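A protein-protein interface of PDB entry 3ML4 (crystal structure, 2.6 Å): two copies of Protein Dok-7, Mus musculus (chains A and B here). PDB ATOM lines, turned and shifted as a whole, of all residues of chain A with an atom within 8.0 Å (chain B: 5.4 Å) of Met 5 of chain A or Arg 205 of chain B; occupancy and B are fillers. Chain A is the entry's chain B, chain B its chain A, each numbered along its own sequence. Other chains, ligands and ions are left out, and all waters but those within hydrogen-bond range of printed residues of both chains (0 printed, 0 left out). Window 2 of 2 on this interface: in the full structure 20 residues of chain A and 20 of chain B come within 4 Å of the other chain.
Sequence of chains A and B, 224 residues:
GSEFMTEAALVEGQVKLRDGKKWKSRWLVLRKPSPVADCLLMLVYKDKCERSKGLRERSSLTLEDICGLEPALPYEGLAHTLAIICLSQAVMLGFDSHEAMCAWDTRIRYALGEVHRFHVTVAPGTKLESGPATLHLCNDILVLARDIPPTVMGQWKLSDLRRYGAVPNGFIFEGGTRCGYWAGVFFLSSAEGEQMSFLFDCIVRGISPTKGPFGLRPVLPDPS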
ATOM      1  N   MET A   5      23.788 -20.576 -26.250  1.00  0.00           N
ATOM      2  CA  MET A   5      23.815 -21.701 -25.272  1.00  0.00           C
ATOM      3  C   MET A   5      24.342 -22.972 -25.927  1.00  0.00           C
ATOM      4  O   MET A   5      23.944 -23.325 -27.039  1.00  0.00           O
ATOM      5  CB  MET A   5      22.423 -21.946 -24.685  1.00  0.00           C
ATOM      6  CG  MET A   5      22.385 -23.050 -23.635  1.00  0.00           C
ATOM      7  SD  MET A   5      20.570 -23.520 -23.102  1.00  0.00           S
ATOM      8  CE  MET A   5      20.206 -22.017 -21.904  1.00  0.00           C
ATOM      9  N   THR A   6      25.230 -23.659 -25.219  1.00  0.00           N
ATOM     10  CA  THR A   6      25.925 -24.812 -25.776  1.00  0.00           C
ATOM     11  C   THR A   6      25.286 -26.125 -25.345  1.00  0.00           C
ATOM     12  O   THR A   6      24.749 -26.237 -24.236  1.00  0.00           O
ATOM     13  CB  THR A   6      27.421 -24.800 -25.402  1.00  0.00           C
ATOM     14  OG1 THR A   6      27.566 -24.503 -24.010  1.00  0.00           O
ATOM     15  CG2 THR A   6      28.167 -23.741 -26.219  1.00  0.00           C
ATOM     16  N   GLU A   7      25.346 -27.110 -26.238  1.00  0.00           N
ATOM     17  CA  GLU A   7      24.817 -28.439 -25.976  1.00  0.00           C
ATOM     18  C   GLU A   7      25.674 -29.166 -24.948  1.00  0.00           C
ATOM     19  O   GLU A   7      26.887 -29.297 -25.118  1.00  0.00           O
ATOM     20  CB  GLU A   7      24.759 -29.241 -27.270  1.00  0.00           C
ATOM     21  CG  GLU A   7      23.784 -30.394 -27.228  1.00  0.00           C
ATOM     22  CD  GLU A   7      23.341 -30.825 -28.605  1.00  0.00           C
ATOM     23  OE1 GLU A   7      23.562 -30.064 -29.571  1.00  0.00           O
ATOM     24  OE2 GLU A   7      22.765 -31.927 -28.721  1.00  0.00           O
ATOM     25  N   ALA A   8      25.031 -29.629 -23.881  1.00  0.00           N
ATOM     26  CA  ALA A   8      25.723 -30.281 -22.777  1.00  0.00           C
ATOM     27  C   ALA A   8      26.161 -31.693 -23.129  1.00  0.00           C
ATOM     28  O   ALA A   8      25.658 -32.296 -24.075  1.00  0.00           O
ATOM     29  CB  ALA A   8      24.844 -30.296 -21.533  1.00  0.00           C
ATOM     30  N   ALA A   9      27.111 -32.204 -22.356  1.00  0.00           N
ATOM     31  CA  ALA A   9      27.604 -33.561 -22.505  1.00  0.00           C
ATOM     32  C   ALA A   9      27.743 -34.172 -21.122  1.00  0.00           C
ATOM     33  O   ALA A   9      28.037 -33.458 -20.165  1.00  0.00           O
ATOM     34  CB  ALA A   9      28.943 -33.544 -23.208  1.00  0.00           C
ATOM     35  N   ARG A  31      25.945 -37.833 -24.650  1.00  0.00           N
ATOM     36  CA  ARG A  31      24.880 -37.294 -23.805  1.00  0.00           C
ATOM     37  C   ARG A  31      23.596 -38.109 -23.916  1.00  0.00           C
ATOM     38  O   ARG A  31      23.341 -38.749 -24.939  1.00  0.00           O
ATOM     39  CB  ARG A  31      24.621 -35.808 -24.110  1.00  0.00           C
ATOM     40  CG  ARG A  31      23.847 -35.482 -25.393  1.00  0.00           C
ATOM     41  CD  ARG A  31      23.571 -33.985 -25.404  1.00  0.00           C
ATOM     42  NE  ARG A  31      22.681 -33.497 -26.456  1.00  0.00           N
ATOM     43  CZ  ARG A  31      21.352 -33.480 -26.373  1.00  0.00           C
ATOM     44  NH1 ARG A  31      20.740 -33.974 -25.307  1.00  0.00           N
ATOM     45  NH2 ARG A  31      20.630 -32.984 -27.370  1.00  0.00           N
ATOM     46  N   LYS A  32      22.807 -38.089 -22.846  1.00  0.00           N
ATOM     47  CA  LYS A  32      21.475 -38.685 -22.841  1.00  0.00           C
ATOM     48  C   LYS A  32      20.539 -37.821 -23.687  1.00  0.00           C
ATOM     49  O   LYS A  32      20.476 -36.608 -23.479  1.00  0.00           O
ATOM     50  CB  LYS A  32      20.949 -38.793 -21.407  1.00  0.00           C
ATOM     51  CG  LYS A  32      21.672 -39.829 -20.552  1.00  0.00           C
ATOM     52  CD  LYS A  32      21.465 -39.589 -19.059  1.00  0.00           C
ATOM     53  CE  LYS A  32      20.235 -40.309 -18.505  1.00  0.00           C
ATOM     54  NZ  LYS A  32      18.959 -39.616 -18.822  1.00  0.00           N
ATOM     55  N   PRO A  33      19.828 -38.439 -24.657  1.00  0.00           N
ATOM     56  CA  PRO A  33      18.880 -37.746 -25.547  1.00  0.00           C
ATOM     57  C   PRO A  33      17.732 -37.086 -24.791  1.00  0.00           C
ATOM     58  O   PRO A  33      17.186 -36.083 -25.249  1.00  0.00           O
ATOM     59  CB  PRO A  33      18.326 -38.876 -26.429  1.00  0.00           C
ATOM     60  CG  PRO A  33      19.343 -39.956 -26.353  1.00  0.00           C
ATOM     61  CD  PRO A  33      19.904 -39.880 -24.968  1.00  0.00           C
ATOM     62  N   LEU A  41      23.169 -40.526 -26.992  1.00  0.00           N
ATOM     63  CA  LEU A  41      23.427 -39.831 -28.240  1.00  0.00           C
ATOM     64  C   LEU A  41      24.927 -39.641 -28.406  1.00  0.00           C
ATOM     65  O   LEU A  41      25.599 -39.079 -27.536  1.00  0.00           O
ATOM     66  CB  LEU A  41      22.699 -38.483 -28.281  1.00  0.00           C
ATOM     67  CG  LEU A  41      22.790 -37.629 -29.553  1.00  0.00           C
ATOM     68  CD1 LEU A  41      22.124 -38.303 -30.740  1.00  0.00           C
ATOM     69  CD2 LEU A  41      22.181 -36.257 -29.314  1.00  0.00           C
ATOM     70  N   LEU A  43      27.734 -37.769 -30.436  1.00  0.00           N
ATOM     71  CA  LEU A  43      27.991 -36.616 -31.293  1.00  0.00           C
ATOM     72  C   LEU A  43      29.478 -36.534 -31.611  1.00  0.00           C
ATOM     73  O   LEU A  43      30.296 -36.300 -30.722  1.00  0.00           O
ATOM     74  CB  LEU A  43      27.485 -35.320 -30.646  1.00  0.00           C
ATOM     75  CG  LEU A  43      25.978 -35.183 -30.369  1.00  0.00           C
ATOM     76  CD1 LEU A  43      25.682 -33.863 -29.669  1.00  0.00           C
ATOM     77  CD2 LEU A  43      25.130 -35.318 -31.635  1.00  0.00           C
ATOM     78  N   ARG A  51      33.924 -28.258 -32.228  1.00  0.00           N
ATOM     79  CA  ARG A  51      33.022 -28.340 -31.078  1.00  0.00           C
ATOM     80  C   ARG A  51      33.029 -27.032 -30.280  1.00  0.00           C
ATOM     81  O   ARG A  51      31.970 -26.547 -29.864  1.00  0.00           O
ATOM     82  CB  ARG A  51      33.412 -29.549 -30.206  1.00  0.00           C
ATOM     83  CG  ARG A  51      33.097 -29.460 -28.713  1.00  0.00           C
ATOM     84  CD  ARG A  51      31.635 -29.738 -28.409  1.00  0.00           C
ATOM     85  NE  ARG A  51      31.416 -29.880 -26.973  1.00  0.00           N
ATOM     86  CZ  ARG A  51      30.262 -29.641 -26.356  1.00  0.00           C
ATOM     87  NH1 ARG A  51      29.205 -29.228 -27.046  1.00  0.00           N
ATOM     88  NH2 ARG A  51      30.171 -29.805 -25.042  1.00  0.00           N
ATOM     89  N   GLY A  54      31.197 -24.466 -31.815  1.00  0.00           N
ATOM     90  CA  GLY A  54      29.790 -24.857 -31.779  1.00  0.00           C
ATOM     91  C   GLY A  54      29.158 -25.072 -33.139  1.00  0.00           C
ATOM     92  O   GLY A  54      28.024 -24.657 -33.365  1.00  0.00           O
ATOM     93  N   TYR B 164      10.984 -23.132 -32.329  1.00  0.00           N
ATOM     94  CA  TYR B 164      10.099 -22.709 -31.250  1.00  0.00           C
ATOM     95  C   TYR B 164      10.636 -21.378 -30.763  1.00  0.00           C
ATOM     96  O   TYR B 164      11.783 -21.027 -31.061  1.00  0.00           O
ATOM     97  CB  TYR B 164      10.089 -23.735 -30.110  1.00  0.00           C
ATOM     98  CG  TYR B 164      11.455 -23.973 -29.531  1.00  0.00           C
ATOM     99  CD1 TYR B 164      11.918 -23.216 -28.460  1.00  0.00           C
ATOM    100  CD2 TYR B 164      12.304 -24.934 -30.078  1.00  0.00           C
ATOM    101  CE1 TYR B 164      13.186 -23.412 -27.943  1.00  0.00           C
ATOM    102  CE2 TYR B 164      13.573 -25.143 -29.563  1.00  0.00           C
ATOM    103  CZ  TYR B 164      14.006 -24.380 -28.496  1.00  0.00           C
ATOM    104  OH  TYR B 164      15.264 -24.581 -27.981  1.00  0.00           O
ATOM    105  N   PHE B 198      12.909 -21.005 -22.554  1.00  0.00           N
ATOM    106  CA  PHE B 198      14.086 -21.415 -21.814  1.00  0.00           C
ATOM    107  C   PHE B 198      14.089 -22.913 -21.485  1.00  0.00           C
ATOM    108  O   PHE B 198      15.138 -23.562 -21.541  1.00  0.00           O
ATOM    109  CB  PHE B 198      14.229 -20.578 -20.539  1.00  0.00           C
ATOM    110  CG  PHE B 198      15.320 -21.055 -19.625  1.00  0.00           C
ATOM    111  CD1 PHE B 198      16.658 -20.968 -20.011  1.00  0.00           C
ATOM    112  CD2 PHE B 198      15.012 -21.604 -18.383  1.00  0.00           C
ATOM    113  CE1 PHE B 198      17.676 -21.419 -19.167  1.00  0.00           C
ATOM    114  CE2 PHE B 198      16.022 -22.054 -17.531  1.00  0.00           C
ATOM    115  CZ  PHE B 198      17.354 -21.960 -17.922  1.00  0.00           C
ATOM    116  N   PHE B 200      12.444 -25.363 -23.214  1.00  0.00           N
ATOM    117  CA  PHE B 200      12.681 -26.021 -24.500  1.00  0.00           C
ATOM    118  C   PHE B 200      14.146 -25.932 -24.911  1.00  0.00           C
ATOM    119  O   PHE B 200      14.705 -26.904 -25.413  1.00  0.00           O
ATOM    120  CB  PHE B 200      11.817 -25.393 -25.594  1.00  0.00           C
ATOM    121  CG  PHE B 200      10.402 -25.887 -25.627  1.00  0.00           C
ATOM    122  CD1 PHE B 200       9.581 -25.787 -24.511  1.00  0.00           C
ATOM    123  CD2 PHE B 200       9.879 -26.416 -26.792  1.00  0.00           C
ATOM    124  CE1 PHE B 200       8.268 -26.228 -24.548  1.00  0.00           C
ATOM    125  CE2 PHE B 200       8.570 -26.861 -26.842  1.00  0.00           C
ATOM    126  CZ  PHE B 200       7.762 -26.768 -25.715  1.00  0.00           C
ATOM    127  N   ASP B 201      14.752 -24.762 -24.701  1.00  0.00           N
ATOM    128  CA  ASP B 201      16.175 -24.542 -24.969  1.00  0.00           C
ATOM    129  C   ASP B 201      17.038 -25.542 -24.204  1.00  0.00           C
ATOM    130  O   ASP B 201      17.909 -26.193 -24.789  1.00  0.00           O
ATOM    131  CB  ASP B 201      16.592 -23.105 -24.609  1.00  0.00           C
ATOM    132  CG  ASP B 201      16.169 -22.084 -25.656  1.00  0.00           C
ATOM    133  OD1 ASP B 201      16.009 -22.437 -26.838  1.00  0.00           O
ATOM    134  OD2 ASP B 201      16.002 -20.907 -25.294  1.00  0.00           O
ATOM    135  N   CYS B 202      16.778 -25.664 -22.903  1.00  0.00           N
ATOM    136  CA  CYS B 202      17.521 -26.579 -22.047  1.00  0.00           C
ATOM    137  C   CYS B 202      17.341 -28.035 -22.487  1.00  0.00           C
ATOM    138  O   CYS B 202      18.327 -28.726 -22.755  1.00  0.00           O
ATOM    139  CB  CYS B 202      17.110 -26.393 -20.588  1.00  0.00           C
ATOM    140  SG  CYS B 202      17.742 -24.891 -19.810  1.00  0.00           S
ATOM    141  N   ILE B 203      16.087 -28.478 -22.587  1.00  0.00           N
ATOM    142  CA  ILE B 203      15.757 -29.880 -22.885  1.00  0.00           C
ATOM    143  C   ILE B 203      16.345 -30.406 -24.206  1.00  0.00           C
ATOM    144  O   ILE B 203      16.969 -31.471 -24.223  1.00  0.00           O
ATOM    145  CB  ILE B 203      14.217 -30.167 -22.754  1.00  0.00           C
ATOM    146  CG1 ILE B 203      13.873 -30.660 -21.345  1.00  0.00           C
ATOM    147  CG2 ILE B 203      13.759 -31.254 -23.717  1.00  0.00           C
ATOM    148  CD1 ILE B 203      14.291 -29.749 -20.210  1.00  0.00           C
ATOM    149  N   VAL B 204      16.166 -29.653 -25.289  1.00  0.00           N
ATOM    150  CA  VAL B 204      16.679 -30.054 -26.612  1.00  0.00           C
ATOM    151  C   VAL B 204      18.209 -30.032 -26.687  1.00  0.00           C
ATOM    152  O   VAL B 204      18.798 -30.535 -27.645  1.00  0.00           O
ATOM    153  CB  VAL B 204      16.078 -29.208 -27.774  1.00  0.00           C
ATOM    154  CG1 VAL B 204      14.555 -29.248 -27.744  1.00  0.00           C
ATOM    155  CG2 VAL B 204      16.595 -27.768 -27.743  1.00  0.00           C
ATOM    156  N   ARG B 205      18.840 -29.449 -25.670  1.00  0.00           N
ATOM    157  CA  ARG B 205      20.299 -29.413 -25.568  1.00  0.00           C
ATOM    158  C   ARG B 205      20.860 -30.321 -24.464  1.00  0.00           C
ATOM    159  O   ARG B 205      22.063 -30.313 -24.200  1.00  0.00           O
ATOM    160  CB  ARG B 205      20.772 -27.973 -25.377  1.00  0.00           C
ATOM    161  CG  ARG B 205      20.756 -27.178 -26.660  1.00  0.00           C
ATOM    162  CD  ARG B 205      20.954 -25.700 -26.404  1.00  0.00           C
ATOM    163  NE  ARG B 205      21.161 -24.978 -27.658  1.00  0.00           N
ATOM    164  CZ  ARG B 205      20.187 -24.547 -28.453  1.00  0.00           C
ATOM    165  NH1 ARG B 205      18.914 -24.749 -28.131  1.00  0.00           N
ATOM    166  NH2 ARG B 205      20.489 -23.909 -29.576  1.00  0.00           N
ATOM    167  N   GLY B 206      19.986 -31.098 -23.825  1.00  0.00           N
ATOM    168  CA  GLY B 206      20.406 -32.055 -22.801  1.00  0.00           C
ATOM    169  C   GLY B 206      20.583 -31.464 -21.414  1.00  0.00           C
ATOM    170  O   GLY B 206      21.165 -32.095 -20.525  1.00  0.00           O
ATOM    171  N   ILE B 207      20.073 -30.252 -21.228  1.00  0.00           N
ATOM    172  CA  ILE B 207      20.215 -29.545 -19.968  1.00  0.00           C
ATOM    173  C   ILE B 207      18.895 -29.575 -19.205  1.00  0.00           C
ATOM    174  O   ILE B 207      17.840 -29.255 -19.755  1.00  0.00           O
ATOM    175  CB  ILE B 207      20.662 -28.073 -20.199  1.00  0.00           C
ATOM    176  CG1 ILE B 207      22.003 -28.026 -20.949  1.00  0.00           C
ATOM    177  CG2 ILE B 207      20.756 -27.311 -18.870  1.00  0.00           C
ATOM    178  CD1 ILE B 207      22.179 -26.811 -21.849  1.00  0.00           C
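Printed residues of chain B that touch a printed residue of chain A: Phe 198, Val 204, Arg 205, Gly 206 and Ile 207. Hydrophobic or aromatic side chains of chain B within 4 Å of the printed part of chain A: Phe 198 and Ile 207. Of the 12 printed residues of chain A, 5 touch a printed residue of chain B. Printed residues of chain A that touch a printed residue of chain B: Met 5, Thr 6, Glu 7, Ala 8 and Arg 31. Among the printed residues, 10 pairs touch across the chains. Among the printed residues, no Asp or Glu carboxylate lies within 4 Å of a Lys or Arg side-chain nitrogen of the other chain.
The backbone carbonyl oxygen of Arg 31 of chain A sits at hydrogen-bond distance from the backbone NH of Leu 41 of chain A (2.7 Å). The backbone carbonyl oxygen (O) of Cys 202 of chain B is in hydrogen-bond range of the backbone NH (N) of Ile 207 of chain B (2.8 Å). The side-chain carboxylate (OE2) of Glu 7 of chain A is in salt-bridge range of the guanidinium group (NH2) of Arg 31 of chain A (2.7 Å). The guanidinium group (NH1) of Arg 51 of chain A lies within hydrogen-bond range of the backbone carbonyl oxygen (O) of Glu 7 of chain A (3.0 Å). The guanidinium group (NH1) of Arg 205 of chain B lies within salt-bridge range of the side-chain carboxylate (OD1) of Asp 201 of chain B (3.9 Å). SG of Cys 202 of chain B lies within hydrogen-bond range of O of Phe 198 of chain B (3.4 Å).
Among the printed residues, pairs that only touch across the chains: Glu 7 of chain A with Arg 205 of chain B (3.5 Å), Thr 6 of chain A with Ile 207 of chain B (3.6 Å), Ala 8 of chain A with Ile 207 of chain B (3.7 Å), Arg 31 of chain A with Arg 205 of chain B (3.7 Å), Met 5 of chain A with Phe 198 of chain B (3.8 Å) and Met 5 of chain A with Ile 207 of chain B (3.9 Å).
Of the printed residues of chain A, Arg 205 of chain B touches Met 5, Glu 7, Ala 8 and Arg 31. Of the printed residues of chain B, Ala 8 of chain A touches Arg 205 (3.1 Å) and Ile 207 (3.7 Å). Printed residues of chain B within 4 Å of Arg 31 of chain A: Val 204 (3.1 Å), Arg 205 (3.7 Å) and Gly 206 (3.2 Å). Leu 41 of chain A touches none of the printed residues of chain B. The nearest residue of chain B that does not touch Met 5 of chain A is Asp 201 of chain B (4.1 Å). The nearest printed residue of chain A that does not touch Phe 198 of chain B is Thr 6 of chain A (9.9 Å).
No position is printed for both chains. Of the 10 pairs that touch across the chains among the printed residues, none has its exchanged pair printed and touching as well.
N of Ala 8 of chain A is in hydrogen-bond range of O of Arg 205 of chain B (3.1 Å). The guanidinium group (NE) of Arg 205 of chain B lies within hydrogen-bond range of the backbone carbonyl oxygen (O) of Met 5 of chain A (3.3 Å). NH1 of Arg 31 of chain A lies close to N of Gly 206 of chain B. The guanidinium group of Arg 31 of chain A lies within hydrogen-bond range of the backbone carbonyl oxygen of Val 204 of chain B (3.1 Å).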
